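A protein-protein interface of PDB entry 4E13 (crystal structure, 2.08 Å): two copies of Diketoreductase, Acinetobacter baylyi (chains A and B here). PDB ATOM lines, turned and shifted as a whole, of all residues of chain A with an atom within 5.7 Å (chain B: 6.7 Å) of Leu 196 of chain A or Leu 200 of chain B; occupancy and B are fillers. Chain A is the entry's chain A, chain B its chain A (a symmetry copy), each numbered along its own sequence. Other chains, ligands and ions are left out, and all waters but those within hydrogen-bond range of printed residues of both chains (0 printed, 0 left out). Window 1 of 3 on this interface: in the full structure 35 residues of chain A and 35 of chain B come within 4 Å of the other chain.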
ATOM      1  N   VAL A 192     -27.752  17.256 -34.799  1.00  0.00           N
ATOM      2  CA  VAL A 192     -26.913  16.590 -33.795  1.00  0.00           C
ATOM      3  C   VAL A 192     -26.497  17.512 -32.641  1.00  0.00           C
ATOM      4  O   VAL A 192     -26.774  17.223 -31.471  1.00  0.00           O
ATOM      5  CB  VAL A 192     -25.649  15.971 -34.415  1.00  0.00           C
ATOM      6  CG1 VAL A 192     -24.811  15.299 -33.323  1.00  0.00           C
ATOM      7  CG2 VAL A 192     -26.023  14.965 -35.497  1.00  0.00           C
ATOM      8  N   LEU A 193     -25.831  18.620 -32.969  1.00  0.00           N
ATOM      9  CA  LEU A 193     -25.227  19.458 -31.934  1.00  0.00           C
ATOM     10  C   LEU A 193     -26.211  19.936 -30.875  1.00  0.00           C
ATOM     11  O   LEU A 193     -25.968  19.769 -29.675  1.00  0.00           O
ATOM     12  CB  LEU A 193     -24.460  20.646 -32.534  1.00  0.00           C
ATOM     13  CG  LEU A 193     -23.825  21.555 -31.477  1.00  0.00           C
ATOM     14  CD1 LEU A 193     -22.988  20.732 -30.500  1.00  0.00           C
ATOM     15  CD2 LEU A 193     -22.989  22.643 -32.137  1.00  0.00           C
ATOM     16  N   ASN A 194     -27.314  20.540 -31.306  1.00  0.00           N
ATOM     17  CA  ASN A 194     -28.282  21.076 -30.354  1.00  0.00           C
ATOM     18  C   ASN A 194     -28.928  19.925 -29.570  1.00  0.00           C
ATOM     19  O   ASN A 194     -29.234  20.063 -28.381  1.00  0.00           O
ATOM     20  CB  ASN A 194     -29.334  21.930 -31.079  1.00  0.00           C
ATOM     21  CG  ASN A 194     -28.706  23.084 -31.888  1.00  0.00           C
ATOM     22  OD1 ASN A 194     -27.568  23.494 -31.637  1.00  0.00           O
ATOM     23  ND2 ASN A 194     -29.452  23.604 -32.865  1.00  0.00           N
ATOM     24  N   SER A 195     -29.115  18.786 -30.234  1.00  0.00           N
ATOM     25  CA  SER A 195     -29.669  17.604 -29.573  1.00  0.00           C
ATOM     26  C   SER A 195     -28.797  17.185 -28.388  1.00  0.00           C
ATOM     27  O   SER A 195     -29.320  16.809 -27.336  1.00  0.00           O
ATOM     28  CB  SER A 195     -29.815  16.441 -30.566  1.00  0.00           C
ATOM     29  OG  SER A 195     -30.668  16.785 -31.652  1.00  0.00           O
ATOM     30  N   LEU A 196     -27.473  17.263 -28.546  1.00  0.00           N
ATOM     31  CA  LEU A 196     -26.536  16.918 -27.458  1.00  0.00           C
ATOM     32  C   LEU A 196     -26.469  18.015 -26.403  1.00  0.00           C
ATOM     33  O   LEU A 196     -26.446  17.747 -25.200  1.00  0.00           O
ATOM     34  CB  LEU A 196     -25.122  16.701 -28.017  1.00  0.00           C
ATOM     35  CG  LEU A 196     -24.988  15.566 -29.031  1.00  0.00           C
ATOM     36  CD1 LEU A 196     -23.589  15.518 -29.620  1.00  0.00           C
ATOM     37  CD2 LEU A 196     -25.354  14.249 -28.358  1.00  0.00           C
ATOM     38  N   LEU A 197     -26.427  19.260 -26.864  1.00  0.00           N
ATOM     39  CA  LEU A 197     -26.125  20.381 -25.986  1.00  0.00           C
ATOM     40  C   LEU A 197     -27.288  20.776 -25.067  1.00  0.00           C
ATOM     41  O   LEU A 197     -27.093  21.040 -23.877  1.00  0.00           O
ATOM     42  CB  LEU A 197     -25.650  21.567 -26.825  1.00  0.00           C
ATOM     43  CG  LEU A 197     -25.192  22.816 -26.077  1.00  0.00           C
ATOM     44  CD1 LEU A 197     -24.067  22.481 -25.106  1.00  0.00           C
ATOM     45  CD2 LEU A 197     -24.743  23.840 -27.105  1.00  0.00           C
ATOM     46  N   VAL A 198     -28.500  20.818 -25.607  1.00  0.00           N
ATOM     47  CA  VAL A 198     -29.637  21.268 -24.806  1.00  0.00           C
ATOM     48  C   VAL A 198     -29.801  20.442 -23.523  1.00  0.00           C
ATOM     49  O   VAL A 198     -30.009  20.993 -22.438  1.00  0.00           O
ATOM     50  CB  VAL A 198     -30.930  21.303 -25.648  1.00  0.00           C
ATOM     51  CG1 VAL A 198     -32.114  21.673 -24.778  1.00  0.00           C
ATOM     52  CG2 VAL A 198     -30.777  22.326 -26.762  1.00  0.00           C
ATOM     53  N   PRO A 199     -29.677  19.111 -23.614  1.00  0.00           N
ATOM     54  CA  PRO A 199     -29.829  18.325 -22.384  1.00  0.00           C
ATOM     55  C   PRO A 199     -28.782  18.652 -21.322  1.00  0.00           C
ATOM     56  O   PRO A 199     -29.085  18.702 -20.124  1.00  0.00           O
ATOM     57  CB  PRO A 199     -29.709  16.878 -22.870  1.00  0.00           C
ATOM     58  CG  PRO A 199     -30.133  16.943 -24.297  1.00  0.00           C
ATOM     59  CD  PRO A 199     -29.607  18.254 -24.809  1.00  0.00           C
ATOM     60  N   LEU A 200     -27.547  18.895 -21.751  1.00  0.00           N
ATOM     61  CA  LEU A 200     -26.505  19.273 -20.797  1.00  0.00           C
ATOM     62  C   LEU A 200     -26.855  20.595 -20.118  1.00  0.00           C
ATOM     63  O   LEU A 200     -26.752  20.733 -18.893  1.00  0.00           O
ATOM     64  CB  LEU A 200     -25.141  19.407 -21.501  1.00  0.00           C
ATOM     65  CG  LEU A 200     -24.014  19.886 -20.585  1.00  0.00           C
ATOM     66  CD1 LEU A 200     -23.884  18.958 -19.380  1.00  0.00           C
ATOM     67  CD2 LEU A 200     -22.690  20.022 -21.346  1.00  0.00           C
ATOM     68  N   TRP A 222     -17.829  20.085 -14.401  1.00  0.00           N
ATOM     69  CA  TRP A 222     -17.870  19.606 -15.770  1.00  0.00           C
ATOM     70  C   TRP A 222     -16.470  19.627 -16.401  1.00  0.00           C
ATOM     71  O   TRP A 222     -16.076  18.664 -17.065  1.00  0.00           O
ATOM     72  CB  TRP A 222     -18.819  20.451 -16.613  1.00  0.00           C
ATOM     73  CG  TRP A 222     -19.007  19.909 -17.996  1.00  0.00           C
ATOM     74  CD1 TRP A 222     -18.569  20.467 -19.174  1.00  0.00           C
ATOM     75  CD2 TRP A 222     -19.691  18.698 -18.361  1.00  0.00           C
ATOM     76  NE1 TRP A 222     -18.942  19.681 -20.242  1.00  0.00           N
ATOM     77  CE2 TRP A 222     -19.630  18.592 -19.773  1.00  0.00           C
ATOM     78  CE3 TRP A 222     -20.351  17.691 -17.629  1.00  0.00           C
ATOM     79  CZ2 TRP A 222     -20.204  17.520 -20.470  1.00  0.00           C
ATOM     80  CZ3 TRP A 222     -20.920  16.632 -18.319  1.00  0.00           C
ATOM     81  CH2 TRP A 222     -20.843  16.554 -19.728  1.00  0.00           C
ATOM     82  N   SER B 195     -25.261  13.996 -12.737  1.00  0.00           N
ATOM     83  CA  SER B 195     -26.455  14.744 -13.131  1.00  0.00           C
ATOM     84  C   SER B 195     -26.243  15.431 -14.481  1.00  0.00           C
ATOM     85  O   SER B 195     -27.151  15.452 -15.315  1.00  0.00           O
ATOM     86  CB  SER B 195     -26.831  15.777 -12.058  1.00  0.00           C
ATOM     87  OG  SER B 195     -27.089  15.157 -10.804  1.00  0.00           O
ATOM     88  N   LEU B 196     -25.046  15.979 -14.707  1.00  0.00           N
ATOM     89  CA  LEU B 196     -24.719  16.637 -15.988  1.00  0.00           C
ATOM     90  C   LEU B 196     -24.457  15.622 -17.093  1.00  0.00           C
ATOM     91  O   LEU B 196     -24.898  15.786 -18.233  1.00  0.00           O
ATOM     92  CB  LEU B 196     -23.468  17.516 -15.835  1.00  0.00           C
ATOM     93  CG  LEU B 196     -23.589  18.654 -14.823  1.00  0.00           C
ATOM     94  CD1 LEU B 196     -22.264  19.377 -14.649  1.00  0.00           C
ATOM     95  CD2 LEU B 196     -24.690  19.607 -15.273  1.00  0.00           C
ATOM     96  N   LEU B 197     -23.722  14.570 -16.750  1.00  0.00           N
ATOM     97  CA  LEU B 197     -23.202  13.653 -17.754  1.00  0.00           C
ATOM     98  C   LEU B 197     -24.261  12.706 -18.334  1.00  0.00           C
ATOM     99  O   LEU B 197     -24.309  12.478 -19.547  1.00  0.00           O
ATOM    100  CB  LEU B 197     -22.023  12.877 -17.167  1.00  0.00           C
ATOM    101  CG  LEU B 197     -21.275  11.927 -18.098  1.00  0.00           C
ATOM    102  CD1 LEU B 197     -20.751  12.671 -19.321  1.00  0.00           C
ATOM    103  CD2 LEU B 197     -20.140  11.296 -17.312  1.00  0.00           C
ATOM    104  N   VAL B 198     -25.112  12.153 -17.480  1.00  0.00           N
ATOM    105  CA  VAL B 198     -26.090  11.177 -17.958  1.00  0.00           C
ATOM    106  C   VAL B 198     -26.967  11.746 -19.083  1.00  0.00           C
ATOM    107  O   VAL B 198     -27.196  11.086 -20.101  1.00  0.00           O
ATOM    108  CB  VAL B 198     -26.930  10.614 -16.792  1.00  0.00           C
ATOM    109  CG1 VAL B 198     -28.003   9.684 -17.317  1.00  0.00           C
ATOM    110  CG2 VAL B 198     -26.019   9.855 -15.840  1.00  0.00           C
ATOM    111  N   PRO B 199     -27.445  12.989 -18.938  1.00  0.00           N
ATOM    112  CA  PRO B 199     -28.280  13.530 -20.018  1.00  0.00           C
ATOM    113  C   PRO B 199     -27.544  13.645 -21.352  1.00  0.00           C
ATOM    114  O   PRO B 199     -28.113  13.379 -22.417  1.00  0.00           O
ATOM    115  CB  PRO B 199     -28.703  14.902 -19.486  1.00  0.00           C
ATOM    116  CG  PRO B 199     -28.630  14.750 -18.005  1.00  0.00           C
ATOM    117  CD  PRO B 199     -27.443  13.863 -17.754  1.00  0.00           C
ATOM    118  N   LEU B 200     -26.270  14.025 -21.305  1.00  0.00           N
ATOM    119  CA  LEU B 200     -25.487  14.099 -22.537  1.00  0.00           C
ATOM    120  C   LEU B 200     -25.368  12.720 -23.181  1.00  0.00           C
ATOM    121  O   LEU B 200     -25.562  12.560 -24.392  1.00  0.00           O
ATOM    122  CB  LEU B 200     -24.077  14.654 -22.255  1.00  0.00           C
ATOM    123  CG  LEU B 200     -23.164  14.681 -23.482  1.00  0.00           C
ATOM    124  CD1 LEU B 200     -23.818  15.479 -24.607  1.00  0.00           C
ATOM    125  CD2 LEU B 200     -21.771  15.219 -23.135  1.00  0.00           C
ATOM    126  N   LEU B 201     -25.027  11.722 -22.373  1.00  0.00           N
ATOM    127  CA  LEU B 201     -24.821  10.373 -22.903  1.00  0.00           C
ATOM    128  C   LEU B 201     -26.132   9.783 -23.419  1.00  0.00           C
ATOM    129  O   LEU B 201     -26.151   9.086 -24.441  1.00  0.00           O
ATOM    130  CB  LEU B 201     -24.200   9.463 -21.841  1.00  0.00           C
ATOM    131  CG  LEU B 201     -22.818   9.898 -21.339  1.00  0.00           C
ATOM    132  CD1 LEU B 201     -22.315   8.936 -20.278  1.00  0.00           C
ATOM    133  CD2 LEU B 201     -21.850   9.966 -22.508  1.00  0.00           C
ATOM    134  N   ASP B 202     -27.226  10.077 -22.718  1.00  0.00           N
ATOM    135  CA  ASP B 202     -28.548   9.633 -23.165  1.00  0.00           C
ATOM    136  C   ASP B 202     -28.913  10.236 -24.508  1.00  0.00           C
ATOM    137  O   ASP B 202     -29.366   9.520 -25.408  1.00  0.00           O
ATOM    138  CB  ASP B 202     -29.631   9.966 -22.136  1.00  0.00           C
ATOM    139  CG  ASP B 202     -29.529   9.116 -20.892  1.00  0.00           C
ATOM    140  OD1 ASP B 202     -28.790   8.107 -20.923  1.00  0.00           O
ATOM    141  OD2 ASP B 202     -30.192   9.455 -19.882  1.00  0.00           O
ATOM    142  N   ALA B 203     -28.696  11.542 -24.657  1.00  0.00           N
ATOM    143  CA  ALA B 203     -29.008  12.203 -25.918  1.00  0.00           C
ATOM    144  C   ALA B 203     -28.189  11.602 -27.051  1.00  0.00           C
ATOM    145  O   ALA B 203     -28.689  11.424 -28.164  1.00  0.00           O
ATOM    146  CB  ALA B 203     -28.777  13.703 -25.826  1.00  0.00           C
ATOM    147  N   ALA B 204     -26.931  11.276 -26.772  1.00  0.00           N
ATOM    148  CA  ALA B 204     -26.094  10.637 -27.781  1.00  0.00           C
ATOM    149  C   ALA B 204     -26.645   9.246 -28.110  1.00  0.00           C
ATOM    150  O   ALA B 204     -26.730   8.859 -29.283  1.00  0.00           O
ATOM    151  CB  ALA B 204     -24.648  10.528 -27.289  1.00  0.00           C
ATOM    152  N   ALA B 205     -27.009   8.491 -27.072  1.00  0.00           N
ATOM    153  CA  ALA B 205     -27.523   7.133 -27.276  1.00  0.00           C
ATOM    154  C   ALA B 205     -28.760   7.153 -28.184  1.00  0.00           C
ATOM    155  O   ALA B 205     -28.856   6.370 -29.133  1.00  0.00           O
ATOM    156  CB  ALA B 205     -27.835   6.469 -25.951  1.00  0.00           C
ATOM    157  N   LEU B 207     -29.642   9.393 -30.430  1.00  0.00           N
ATOM    158  CA  LEU B 207     -29.237   9.663 -31.802  1.00  0.00           C
ATOM    159  C   LEU B 207     -28.732   8.405 -32.490  1.00  0.00           C
ATOM    160  O   LEU B 207     -28.981   8.205 -33.684  1.00  0.00           O
ATOM    161  CB  LEU B 207     -28.140  10.736 -31.865  1.00  0.00           C
ATOM    162  CG  LEU B 207     -28.513  12.142 -31.401  1.00  0.00           C
ATOM    163  CD1 LEU B 207     -27.291  13.060 -31.496  1.00  0.00           C
ATOM    164  CD2 LEU B 207     -29.640  12.669 -32.284  1.00  0.00           C
ATOM    165  N   THR B 217     -19.524  10.562 -36.056  1.00  0.00           N
ATOM    166  CA  THR B 217     -20.203  11.810 -36.349  1.00  0.00           C
ATOM    167  C   THR B 217     -20.658  12.518 -35.085  1.00  0.00           C
ATOM    168  O   THR B 217     -20.407  13.713 -34.901  1.00  0.00           O
ATOM    169  CB  THR B 217     -21.419  11.579 -37.250  1.00  0.00           C
ATOM    170  OG1 THR B 217     -20.972  11.100 -38.520  1.00  0.00           O
ATOM    171  CG2 THR B 217     -22.191  12.870 -37.447  1.00  0.00           C
ATOM    172  N   ILE B 218     -21.332  11.783 -34.213  1.00  0.00           N
ATOM    173  CA  ILE B 218     -21.829  12.359 -32.979  1.00  0.00           C
ATOM    174  C   ILE B 218     -20.658  12.876 -32.141  1.00  0.00           C
ATOM    175  O   ILE B 218     -20.723  13.970 -31.570  1.00  0.00           O
ATOM    176  CB  ILE B 218     -22.649  11.309 -32.177  1.00  0.00           C
ATOM    177  CG1 ILE B 218     -23.835  10.826 -33.026  1.00  0.00           C
ATOM    178  CG2 ILE B 218     -23.134  11.902 -30.874  1.00  0.00           C
ATOM    179  CD1 ILE B 218     -24.689   9.744 -32.373  1.00  0.00           C
ATOM    180  N   ASP B 219     -19.586  12.090 -32.066  1.00  0.00           N
ATOM    181  CA  ASP B 219     -18.427  12.509 -31.299  1.00  0.00           C
ATOM    182  C   ASP B 219     -17.741  13.745 -31.879  1.00  0.00           C
ATOM    183  O   ASP B 219     -17.452  14.689 -31.139  1.00  0.00           O
ATOM    184  CB  ASP B 219     -17.445  11.363 -31.095  1.00  0.00           C
ATOM    185  CG  ASP B 219     -17.907  10.384 -30.023  1.00  0.00           C
ATOM    186  OD1 ASP B 219     -18.888  10.697 -29.298  1.00  0.00           O
ATOM    187  OD2 ASP B 219     -17.273   9.311 -29.891  1.00  0.00           O
ATOM    188  N   THR B 221     -18.988  16.006 -33.703  1.00  0.00           N
ATOM    189  CA  THR B 221     -19.889  17.137 -33.556  1.00  0.00           C
ATOM    190  C   THR B 221     -19.742  17.747 -32.166  1.00  0.00           C
ATOM    191  O   THR B 221     -19.770  18.969 -32.003  1.00  0.00           O
ATOM    192  CB  THR B 221     -21.368  16.732 -33.773  1.00  0.00           C
ATOM    193  OG1 THR B 221     -21.539  16.238 -35.103  1.00  0.00           O
ATOM    194  CG2 THR B 221     -22.286  17.925 -33.550  1.00  0.00           C
ATOM    195  N   TRP B 222     -19.592  16.903 -31.153  1.00  0.00           N
ATOM    196  CA  TRP B 222     -19.461  17.404 -29.797  1.00  0.00           C
ATOM    197  C   TRP B 222     -18.093  18.069 -29.588  1.00  0.00           C
ATOM    198  O   TRP B 222     -18.015  19.150 -28.996  1.00  0.00           O
ATOM    199  CB  TRP B 222     -19.638  16.280 -28.782  1.00  0.00           C
ATOM    200  CG  TRP B 222     -19.657  16.770 -27.368  1.00  0.00           C
ATOM    201  CD1 TRP B 222     -18.701  16.558 -26.403  1.00  0.00           C
ATOM    202  CD2 TRP B 222     -20.684  17.556 -26.743  1.00  0.00           C
ATOM    203  NE1 TRP B 222     -19.076  17.158 -25.221  1.00  0.00           N
ATOM    204  CE2 TRP B 222     -20.285  17.776 -25.401  1.00  0.00           C
ATOM    205  CE3 TRP B 222     -21.908  18.096 -27.188  1.00  0.00           C
ATOM    206  CZ2 TRP B 222     -21.064  18.513 -24.497  1.00  0.00           C
ATOM    207  CZ3 TRP B 222     -22.678  18.823 -26.293  1.00  0.00           C
ATOM    208  CH2 TRP B 222     -22.253  19.026 -24.961  1.00  0.00           C
ATOM    209  N   LYS B 230     -13.152  14.868 -25.720  1.00  0.00           N
ATOM    210  CA  LYS B 230     -13.757  13.581 -26.052  1.00  0.00           C
ATOM    211  C   LYS B 230     -15.281  13.660 -26.241  1.00  0.00           C
ATOM    212  O   LYS B 230     -15.991  14.329 -25.481  1.00  0.00           O
ATOM    213  CB  LYS B 230     -13.407  12.533 -24.989  1.00  0.00           C
ATOM    214  CG  LYS B 230     -11.907  12.206 -24.909  1.00  0.00           C
ATOM    215  CD  LYS B 230     -11.611  11.227 -23.799  1.00  0.00           C
ATOM    216  CE  LYS B 230     -10.097  11.027 -23.628  1.00  0.00           C
ATOM    217  NZ  LYS B 230      -9.444  10.645 -24.925  1.00  0.00           N
ATOM    218  N   GLY B 231     -15.763  12.958 -27.265  1.00  0.00           N
ATOM    219  CA  GLY B 231     -17.190  12.896 -27.548  1.00  0.00           C
ATOM    220  C   GLY B 231     -17.914  11.881 -26.682  1.00  0.00           C
ATOM    221  O   GLY B 231     -17.270  11.092 -25.982  1.00  0.00           O
ATOM    222  N   PRO B 232     -19.254  11.857 -26.717  1.00  0.00           N
ATOM    223  CA  PRO B 232     -20.017  10.916 -25.885  1.00  0.00           C
ATOM    224  C   PRO B 232     -19.577   9.461 -25.973  1.00  0.00           C
ATOM    225  O   PRO B 232     -19.442   8.779 -24.954  1.00  0.00           O
ATOM    226  CB  PRO B 232     -21.462  11.116 -26.355  1.00  0.00           C
ATOM    227  CG  PRO B 232     -21.480  12.533 -26.888  1.00  0.00           C
ATOM    228  CD  PRO B 232     -20.132  12.703 -27.545  1.00  0.00           C
ATOM    229  N   ILE B 235     -16.490   8.706 -24.336  1.00  0.00           N
ATOM    230  CA  ILE B 235     -16.753   8.691 -22.904  1.00  0.00           C
ATOM    231  C   ILE B 235     -17.390   7.362 -22.504  1.00  0.00           C
ATOM    232  O   ILE B 235     -16.991   6.765 -21.500  1.00  0.00           O
ATOM    233  CB  ILE B 235     -17.621   9.896 -22.463  1.00  0.00           C
ATOM    234  CG1 ILE B 235     -16.865  11.196 -22.764  1.00  0.00           C
ATOM    235  CG2 ILE B 235     -17.925   9.818 -20.970  1.00  0.00           C
ATOM    236  CD1 ILE B 235     -17.626  12.476 -22.424  1.00  0.00           C
ATOM    237  N   PHE B 236     -18.353   6.869 -23.286  1.00  0.00           N
ATOM    238  CA  PHE B 236     -18.892   5.524 -23.009  1.00  0.00           C
ATOM    239  C   PHE B 236     -17.768   4.495 -22.860  1.00  0.00           C
ATOM    240  O   PHE B 236     -17.776   3.691 -21.927  1.00  0.00           O
ATOM    241  CB  PHE B 236     -19.879   5.042 -24.086  1.00  0.00           C
ATOM    242  CG  PHE B 236     -21.295   5.507 -23.881  1.00  0.00           C
ATOM    243  CD1 PHE B 236     -21.976   6.181 -24.890  1.00  0.00           C
ATOM    244  CD2 PHE B 236     -21.949   5.265 -22.681  1.00  0.00           C
ATOM    245  CE1 PHE B 236     -23.303   6.613 -24.707  1.00  0.00           C
ATOM    246  CE2 PHE B 236     -23.283   5.693 -22.478  1.00  0.00           C
ATOM    247  CZ  PHE B 236     -23.956   6.366 -23.491  1.00  0.00           C
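The backbone carbonyl oxygen (O) of Thr 217 of chain B sits at hydrogen-bond distance from the side-chain hydroxyl (OG1) of Thr 221 of chain B, at 2.8 Å.
Among the printed residues, merely in contact across the chains: Val 192 of chain A with Leu 207 of chain B (3.8 Å), Val 192 of chain A with Thr 221 of chain B (3.7 Å), Leu 193 of chain A with Thr 221 of chain B (3.6 Å), Ser 195 of chain A with Ala 203 of chain B (3.5 Å), Leu 196 of chain A with Leu 200 of chain B (3.5 Å), Leu 196 of chain A with Ala 204 of chain B (3.7 Å), Leu 196 of chain A with Leu 207 of chain B (3.9 Å), Leu 196 of chain A with Ile 218 of chain B (3.8 Å), Leu 196 of chain A with Trp 222 of chain B (3.6 Å), Leu 197 of chain A with Trp 222 of chain B (3.8 Å), Pro 199 of chain A with Pro 199 of chain B (3.9 Å), Pro 199 of chain A with Ala 203 of chain B (3.8 Å), Leu 200 of chain A with Leu 196 of chain B (3.5 Å), Leu 200 of chain A with Trp 222 of chain B (3.8 Å), Trp 222 of chain A with Leu 196 of chain B (3.6 Å), Trp 222 of chain A with Leu 197 of chain B (3.8 Å) and Trp 222 of chain A with Leu 200 of chain B (3.8 Å).
Leu 200 of chain B touches just these residues of chain A: Leu 196 and Trp 222.
Printed residues of chain B within 4 Å of Val 192 of chain A: Leu 207 (3.8 Å) and Thr 221 (3.7 Å).
Printed residues of chain B within 4 Å of Leu 193 of chain A: Thr 221 (3.6 Å).
Of the printed residues of chain B, Trp 222 of chain A touches Leu 196 (3.6 Å), Leu 197 (3.8 Å) and Leu 200 (3.8 Å).
Printed residues of chain A within 4 Å of Leu 207 of chain B: Val 192 and Leu 196.
The nearest residue of chain B that does not touch Leu 196 of chain A is Ala 203 of chain B (4.1 Å).
The nearest residue of chain A that does not touch Leu 200 of chain B is Pro 199 of chain A (4.7 Å).
The nearest printed residue of chain B that does not touch Ser 195 of chain A is Leu 207 of chain B (4.1 Å).
Of the 10 printed residues of chain A, 8 touch a printed residue of chain B.
Among the printed residues, 17 pairs touch across the chains.
Leu 196 of chain A touches Leu 200 of chain B, and with the chains exchanged Leu 200 of chain A touches Leu 196 of chain B.
Leu 196 of chain A touches Trp 222 of chain B, and with the chains exchanged Trp 222 of chain A touches Leu 196 of chain B.
Pro 199 of chain A touches its own counterpart, Pro 199 of chain B.
Leu 200 of chain A touches Trp 222 of chain B, and with the chains exchanged Trp 222 of chain A touches Leu 200 of chain B.
7 positions are printed for both chains.
Of the 17 pairs that touch across the chains among the printed residues, 9 have their exchanged pair printed and touching as well.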
